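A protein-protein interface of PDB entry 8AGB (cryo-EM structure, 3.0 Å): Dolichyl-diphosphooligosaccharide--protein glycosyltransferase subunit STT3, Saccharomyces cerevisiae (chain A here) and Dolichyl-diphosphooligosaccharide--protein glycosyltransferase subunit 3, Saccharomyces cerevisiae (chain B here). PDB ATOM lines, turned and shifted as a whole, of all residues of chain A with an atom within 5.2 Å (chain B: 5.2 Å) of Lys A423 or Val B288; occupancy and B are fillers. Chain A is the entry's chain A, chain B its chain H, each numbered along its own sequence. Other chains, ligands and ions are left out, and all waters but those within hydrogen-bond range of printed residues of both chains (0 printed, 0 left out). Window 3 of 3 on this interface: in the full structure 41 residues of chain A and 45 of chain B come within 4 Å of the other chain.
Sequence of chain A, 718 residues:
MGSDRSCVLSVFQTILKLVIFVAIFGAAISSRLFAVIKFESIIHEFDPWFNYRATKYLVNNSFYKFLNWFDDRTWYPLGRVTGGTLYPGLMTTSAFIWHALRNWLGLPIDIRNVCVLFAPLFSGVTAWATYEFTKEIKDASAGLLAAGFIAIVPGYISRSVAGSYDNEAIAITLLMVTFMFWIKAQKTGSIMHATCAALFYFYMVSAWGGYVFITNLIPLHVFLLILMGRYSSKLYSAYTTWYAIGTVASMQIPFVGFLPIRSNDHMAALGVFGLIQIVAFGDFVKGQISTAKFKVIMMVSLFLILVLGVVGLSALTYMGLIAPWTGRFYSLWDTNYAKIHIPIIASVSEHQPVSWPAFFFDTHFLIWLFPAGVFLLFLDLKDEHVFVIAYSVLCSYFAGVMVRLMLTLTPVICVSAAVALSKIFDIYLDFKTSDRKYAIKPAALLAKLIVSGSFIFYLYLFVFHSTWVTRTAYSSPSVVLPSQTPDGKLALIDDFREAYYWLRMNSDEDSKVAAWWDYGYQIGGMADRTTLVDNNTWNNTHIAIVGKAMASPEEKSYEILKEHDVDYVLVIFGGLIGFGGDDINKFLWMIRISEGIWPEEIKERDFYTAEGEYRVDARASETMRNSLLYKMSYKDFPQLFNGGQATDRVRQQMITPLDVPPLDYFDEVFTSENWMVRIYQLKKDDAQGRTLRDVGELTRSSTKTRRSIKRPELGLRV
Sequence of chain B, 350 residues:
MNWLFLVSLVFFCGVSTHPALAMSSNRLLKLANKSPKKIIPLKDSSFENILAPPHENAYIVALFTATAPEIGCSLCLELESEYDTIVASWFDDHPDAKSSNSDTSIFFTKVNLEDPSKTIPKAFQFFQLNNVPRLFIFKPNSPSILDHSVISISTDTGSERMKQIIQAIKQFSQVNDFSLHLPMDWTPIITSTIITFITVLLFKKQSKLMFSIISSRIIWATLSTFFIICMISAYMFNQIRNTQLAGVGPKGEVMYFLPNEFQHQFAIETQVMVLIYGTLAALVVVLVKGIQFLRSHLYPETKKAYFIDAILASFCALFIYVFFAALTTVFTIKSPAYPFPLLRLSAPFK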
ATOM      1  N   LYS A 138       2.160 -23.004 -18.747  1.00  0.00           N
ATOM      2  CA  LYS A 138       3.265 -23.424 -17.897  1.00  0.00           C
ATOM      3  C   LYS A 138       3.131 -22.924 -16.463  1.00  0.00           C
ATOM      4  O   LYS A 138       2.665 -23.655 -15.584  1.00  0.00           O
ATOM      5  CB  LYS A 138       4.595 -22.950 -18.478  1.00  0.00           C
ATOM      6  CG  LYS A 138       5.789 -23.649 -17.868  1.00  0.00           C
ATOM      7  CD  LYS A 138       7.076 -23.267 -18.556  1.00  0.00           C
ATOM      8  CE  LYS A 138       8.260 -23.748 -17.748  1.00  0.00           C
ATOM      9  NZ  LYS A 138       8.257 -23.153 -16.386  1.00  0.00           N
ATOM     10  N   LEU A 376      10.352 -28.183 -26.869  1.00  0.00           N
ATOM     11  CA  LEU A 376      10.192 -28.496 -25.457  1.00  0.00           C
ATOM     12  C   LEU A 376       8.721 -28.729 -25.138  1.00  0.00           C
ATOM     13  O   LEU A 376       8.396 -29.509 -24.237  1.00  0.00           O
ATOM     14  CB  LEU A 376      10.770 -27.373 -24.599  1.00  0.00           C
ATOM     15  CG  LEU A 376      12.298 -27.295 -24.595  1.00  0.00           C
ATOM     16  CD1 LEU A 376      12.772 -26.035 -23.897  1.00  0.00           C
ATOM     17  CD2 LEU A 376      12.893 -28.531 -23.946  1.00  0.00           C
ATOM     18  N   LEU A 377       7.817 -28.063 -25.872  1.00  0.00           N
ATOM     19  CA  LEU A 377       6.389 -28.215 -25.642  1.00  0.00           C
ATOM     20  C   LEU A 377       5.868 -29.456 -26.338  1.00  0.00           C
ATOM     21  O   LEU A 377       4.686 -29.787 -26.208  1.00  0.00           O
ATOM     22  CB  LEU A 377       5.631 -26.978 -26.120  1.00  0.00           C
ATOM     23  CG  LEU A 377       5.556 -25.848 -25.095  1.00  0.00           C
ATOM     24  CD1 LEU A 377       4.576 -24.788 -25.543  1.00  0.00           C
ATOM     25  CD2 LEU A 377       5.177 -26.387 -23.727  1.00  0.00           C
ATOM     26  N   ASP A 380       6.571 -32.760 -23.445  1.00  0.00           N
ATOM     27  CA  ASP A 380       5.618 -33.050 -22.380  1.00  0.00           C
ATOM     28  C   ASP A 380       4.253 -33.414 -22.959  1.00  0.00           C
ATOM     29  O   ASP A 380       3.569 -34.298 -22.432  1.00  0.00           O
ATOM     30  CB  ASP A 380       5.521 -31.842 -21.442  1.00  0.00           C
ATOM     31  CG  ASP A 380       4.634 -32.089 -20.230  1.00  0.00           C
ATOM     32  OD1 ASP A 380       4.094 -33.203 -20.073  1.00  0.00           O
ATOM     33  OD2 ASP A 380       4.492 -31.155 -19.415  1.00  0.00           O
ATOM     34  N   ALA A 418       8.748 -17.343 -24.429  1.00  0.00           N
ATOM     35  CA  ALA A 418       8.603 -17.254 -22.982  1.00  0.00           C
ATOM     36  C   ALA A 418       8.782 -18.622 -22.347  1.00  0.00           C
ATOM     37  O   ALA A 418       9.533 -18.779 -21.385  1.00  0.00           O
ATOM     38  CB  ALA A 418       7.242 -16.664 -22.624  1.00  0.00           C
ATOM     39  N   VAL A 419       7.984 -19.592 -22.801  1.00  0.00           N
ATOM     40  CA  VAL A 419       8.039 -20.956 -22.267  1.00  0.00           C
ATOM     41  C   VAL A 419       9.480 -21.454 -22.227  1.00  0.00           C
ATOM     42  O   VAL A 419       9.981 -21.887 -21.183  1.00  0.00           O
ATOM     43  CB  VAL A 419       7.144 -21.896 -23.091  1.00  0.00           C
ATOM     44  CG1 VAL A 419       7.484 -23.342 -22.792  1.00  0.00           C
ATOM     45  CG2 VAL A 419       5.685 -21.627 -22.793  1.00  0.00           C
ATOM     46  N   ALA A 420      10.128 -21.481 -23.394  1.00  0.00           N
ATOM     47  CA  ALA A 420      11.525 -21.902 -23.511  1.00  0.00           C
ATOM     48  C   ALA A 420      12.412 -21.222 -22.472  1.00  0.00           C
ATOM     49  O   ALA A 420      13.110 -21.885 -21.690  1.00  0.00           O
ATOM     50  CB  ALA A 420      12.036 -21.619 -24.924  1.00  0.00           C
ATOM     51  N   LEU A 421      12.460 -19.888 -22.522  1.00  0.00           N
ATOM     52  CA  LEU A 421      13.300 -19.119 -21.608  1.00  0.00           C
ATOM     53  C   LEU A 421      13.015 -19.497 -20.162  1.00  0.00           C
ATOM     54  O   LEU A 421      13.940 -19.664 -19.360  1.00  0.00           O
ATOM     55  CB  LEU A 421      13.085 -17.623 -21.831  1.00  0.00           C
ATOM     56  CG  LEU A 421      14.177 -16.703 -21.287  1.00  0.00           C
ATOM     57  CD1 LEU A 421      15.546 -17.320 -21.488  1.00  0.00           C
ATOM     58  CD2 LEU A 421      14.102 -15.347 -21.953  1.00  0.00           C
ATOM     59  N   SER A 422      11.734 -19.535 -19.793  1.00  0.00           N
ATOM     60  CA  SER A 422      11.336 -19.911 -18.442  1.00  0.00           C
ATOM     61  C   SER A 422      11.943 -21.250 -18.060  1.00  0.00           C
ATOM     62  O   SER A 422      12.461 -21.411 -16.953  1.00  0.00           O
ATOM     63  CB  SER A 422       9.813 -19.954 -18.336  1.00  0.00           C
ATOM     64  OG  SER A 422       9.410 -20.779 -17.260  1.00  0.00           O
ATOM     65  N   LYS A 423      11.789 -22.253 -18.928  1.00  0.00           N
ATOM     66  CA  LYS A 423      12.379 -23.566 -18.673  1.00  0.00           C
ATOM     67  C   LYS A 423      13.866 -23.443 -18.367  1.00  0.00           C
ATOM     68  O   LYS A 423      14.361 -24.010 -17.387  1.00  0.00           O
ATOM     69  CB  LYS A 423      12.154 -24.498 -19.861  1.00  0.00           C
ATOM     70  CG  LYS A 423      10.702 -24.772 -20.182  1.00  0.00           C
ATOM     71  CD  LYS A 423      10.480 -26.242 -20.488  1.00  0.00           C
ATOM     72  CE  LYS A 423       9.029 -26.521 -20.822  1.00  0.00           C
ATOM     73  NZ  LYS A 423       8.649 -27.918 -20.491  1.00  0.00           N
ATOM     74  N   ILE A 424      14.601 -22.740 -19.236  1.00  0.00           N
ATOM     75  CA  ILE A 424      16.036 -22.530 -19.019  1.00  0.00           C
ATOM     76  C   ILE A 424      16.287 -21.952 -17.630  1.00  0.00           C
ATOM     77  O   ILE A 424      17.110 -22.459 -16.850  1.00  0.00           O
ATOM     78  CB  ILE A 424      16.616 -21.612 -20.111  1.00  0.00           C
ATOM     79  CG1 ILE A 424      16.859 -22.388 -21.402  1.00  0.00           C
ATOM     80  CG2 ILE A 424      17.911 -20.978 -19.643  1.00  0.00           C
ATOM     81  CD1 ILE A 424      17.381 -21.534 -22.532  1.00  0.00           C
ATOM     82  N   PHE A 425      15.596 -20.855 -17.318  1.00  0.00           N
ATOM     83  CA  PHE A 425      15.766 -20.199 -16.028  1.00  0.00           C
ATOM     84  C   PHE A 425      15.494 -21.164 -14.884  1.00  0.00           C
ATOM     85  O   PHE A 425      16.201 -21.149 -13.869  1.00  0.00           O
ATOM     86  CB  PHE A 425      14.849 -18.983 -15.945  1.00  0.00           C
ATOM     87  CG  PHE A 425      15.378 -17.777 -16.666  1.00  0.00           C
ATOM     88  CD1 PHE A 425      16.716 -17.687 -17.003  1.00  0.00           C
ATOM     89  CD2 PHE A 425      14.539 -16.730 -16.998  1.00  0.00           C
ATOM     90  CE1 PHE A 425      17.205 -16.580 -17.662  1.00  0.00           C
ATOM     91  CE2 PHE A 425      15.023 -15.620 -17.654  1.00  0.00           C
ATOM     92  CZ  PHE A 425      16.357 -15.545 -17.987  1.00  0.00           C
ATOM     93  N   ASP A 426      14.458 -21.995 -15.020  1.00  0.00           N
ATOM     94  CA  ASP A 426      14.067 -22.926 -13.967  1.00  0.00           C
ATOM     95  C   ASP A 426      15.226 -23.803 -13.525  1.00  0.00           C
ATOM     96  O   ASP A 426      15.186 -24.371 -12.429  1.00  0.00           O
ATOM     97  CB  ASP A 426      12.906 -23.801 -14.440  1.00  0.00           C
ATOM     98  CG  ASP A 426      11.555 -23.232 -14.063  1.00  0.00           C
ATOM     99  OD1 ASP A 426      11.478 -22.497 -13.059  1.00  0.00           O
ATOM    100  OD2 ASP A 426      10.568 -23.521 -14.769  1.00  0.00           O
ATOM    101  N   ILE A 427      16.253 -23.930 -14.361  1.00  0.00           N
ATOM    102  CA  ILE A 427      17.417 -24.740 -14.060  1.00  0.00           C
ATOM    103  C   ILE A 427      18.612 -23.873 -13.692  1.00  0.00           C
ATOM    104  O   ILE A 427      19.397 -24.237 -12.816  1.00  0.00           O
ATOM    105  CB  ILE A 427      17.762 -25.675 -15.239  1.00  0.00           C
ATOM    106  CG1 ILE A 427      16.502 -26.356 -15.771  1.00  0.00           C
ATOM    107  CG2 ILE A 427      18.784 -26.713 -14.810  1.00  0.00           C
ATOM    108  CD1 ILE A 427      16.783 -27.559 -16.639  1.00  0.00           C
ATOM    109  N   LEU B 283      20.901 -26.022 -29.594  1.00  0.00           N
ATOM    110  CA  LEU B 283      21.718 -25.846 -28.403  1.00  0.00           C
ATOM    111  C   LEU B 283      20.859 -25.630 -27.168  1.00  0.00           C
ATOM    112  O   LEU B 283      21.084 -26.274 -26.135  1.00  0.00           O
ATOM    113  CB  LEU B 283      22.682 -24.678 -28.593  1.00  0.00           C
ATOM    114  CG  LEU B 283      23.864 -24.911 -29.531  1.00  0.00           C
ATOM    115  CD1 LEU B 283      24.144 -23.664 -30.345  1.00  0.00           C
ATOM    116  CD2 LEU B 283      25.092 -25.327 -28.745  1.00  0.00           C
ATOM    117  N   VAL B 284      19.811 -24.808 -27.276  1.00  0.00           N
ATOM    118  CA  VAL B 284      19.026 -24.521 -26.080  1.00  0.00           C
ATOM    119  C   VAL B 284      18.365 -25.797 -25.586  1.00  0.00           C
ATOM    120  O   VAL B 284      18.328 -26.062 -24.379  1.00  0.00           O
ATOM    121  CB  VAL B 284      18.007 -23.388 -26.322  1.00  0.00           C
ATOM    122  CG1 VAL B 284      18.196 -22.756 -27.679  1.00  0.00           C
ATOM    123  CG2 VAL B 284      16.581 -23.867 -26.116  1.00  0.00           C
ATOM    124  N   VAL B 285      17.911 -26.649 -26.512  1.00  0.00           N
ATOM    125  CA  VAL B 285      17.255 -27.876 -26.080  1.00  0.00           C
ATOM    126  C   VAL B 285      18.244 -28.720 -25.300  1.00  0.00           C
ATOM    127  O   VAL B 285      17.940 -29.200 -24.199  1.00  0.00           O
ATOM    128  CB  VAL B 285      16.675 -28.639 -27.283  1.00  0.00           C
ATOM    129  CG1 VAL B 285      16.097 -29.965 -26.832  1.00  0.00           C
ATOM    130  CG2 VAL B 285      15.618 -27.803 -27.975  1.00  0.00           C
ATOM    131  N   VAL B 286      19.489 -28.777 -25.782  1.00  0.00           N
ATOM    132  CA  VAL B 286      20.515 -29.532 -25.077  1.00  0.00           C
ATOM    133  C   VAL B 286      20.665 -28.962 -23.679  1.00  0.00           C
ATOM    134  O   VAL B 286      20.753 -29.697 -22.690  1.00  0.00           O
ATOM    135  CB  VAL B 286      21.841 -29.506 -25.857  1.00  0.00           C
ATOM    136  CG1 VAL B 286      23.021 -29.606 -24.913  1.00  0.00           C
ATOM    137  CG2 VAL B 286      21.876 -30.637 -26.862  1.00  0.00           C
ATOM    138  N   LEU B 287      20.706 -27.634 -23.586  1.00  0.00           N
ATOM    139  CA  LEU B 287      20.870 -26.992 -22.293  1.00  0.00           C
ATOM    140  C   LEU B 287      19.748 -27.412 -21.352  1.00  0.00           C
ATOM    141  O   LEU B 287      19.992 -27.755 -20.190  1.00  0.00           O
ATOM    142  CB  LEU B 287      20.894 -25.475 -22.480  1.00  0.00           C
ATOM    143  CG  LEU B 287      21.654 -24.617 -21.475  1.00  0.00           C
ATOM    144  CD1 LEU B 287      23.056 -25.157 -21.280  1.00  0.00           C
ATOM    145  CD2 LEU B 287      21.695 -23.178 -21.952  1.00  0.00           C
ATOM    146  N   VAL B 288      18.503 -27.387 -21.841  1.00  0.00           N
ATOM    147  CA  VAL B 288      17.371 -27.697 -20.970  1.00  0.00           C
ATOM    148  C   VAL B 288      17.273 -29.192 -20.702  1.00  0.00           C
ATOM    149  O   VAL B 288      17.054 -29.620 -19.563  1.00  0.00           O
ATOM    150  CB  VAL B 288      16.060 -27.158 -21.567  1.00  0.00           C
ATOM    151  CG1 VAL B 288      14.967 -27.178 -20.520  1.00  0.00           C
ATOM    152  CG2 VAL B 288      16.251 -25.761 -22.085  1.00  0.00           C
ATOM    153  N   LYS B 289      17.436 -30.011 -21.739  1.00  0.00           N
ATOM    154  CA  LYS B 289      17.168 -31.436 -21.611  1.00  0.00           C
ATOM    155  C   LYS B 289      18.416 -32.301 -21.520  1.00  0.00           C
ATOM    156  O   LYS B 289      18.695 -32.886 -20.468  1.00  0.00           O
ATOM    157  CB  LYS B 289      16.314 -31.900 -22.792  1.00  0.00           C
ATOM    158  CG  LYS B 289      15.063 -32.660 -22.394  1.00  0.00           C
ATOM    159  CD  LYS B 289      14.055 -31.748 -21.718  1.00  0.00           C
ATOM    160  CE  LYS B 289      12.963 -32.550 -21.027  1.00  0.00           C
ATOM    161  NZ  LYS B 289      11.937 -31.674 -20.401  1.00  0.00           N
ATOM    162  N   GLY B 290      19.170 -32.395 -22.610  1.00  0.00           N
ATOM    163  CA  GLY B 290      20.232 -33.377 -22.677  1.00  0.00           C
ATOM    164  C   GLY B 290      21.591 -33.017 -22.116  1.00  0.00           C
ATOM    165  O   GLY B 290      22.605 -33.486 -22.640  1.00  0.00           O
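Hydrophobic or aromatic side chains of chain B within 4 Å of the printed part of chain A: Val B288. Among the printed residues, 4 pairs touch across the chains. Among the printed residues, no Asp or Glu carboxylate lies within 4 Å of a Lys or Arg side-chain nitrogen of the other chain.
Among the printed residues, pairs that only touch across the chains: Leu A376 with Val B288 (3.9 Å), Lys A423 with Val B288 (3.9 Å), Ile A424 with Val B288 (3.5 Å) and Ile A427 with Val B288 (3.6 Å).
Of the printed residues of chain B, Leu A376 touches Val B288. Lys A423 touches one residue of chain B. Of the printed residues of chain B, Ile A424 touches Val B288. Of the printed residues of chain B, Ile A427 touches Val B288 (3.6 Å). Val B288 touches just these residues of chain A: Leu A376, Lys A423, Ile A424 and Ile A427. Lys B289 touches none of the printed residues of chain A. The nearest residue of chain B that does not touch Lys A423 is Lys B289 (5.0 Å). The nearest residue of chain A that does not touch Val B288 is Ala A420 (5.0 Å).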
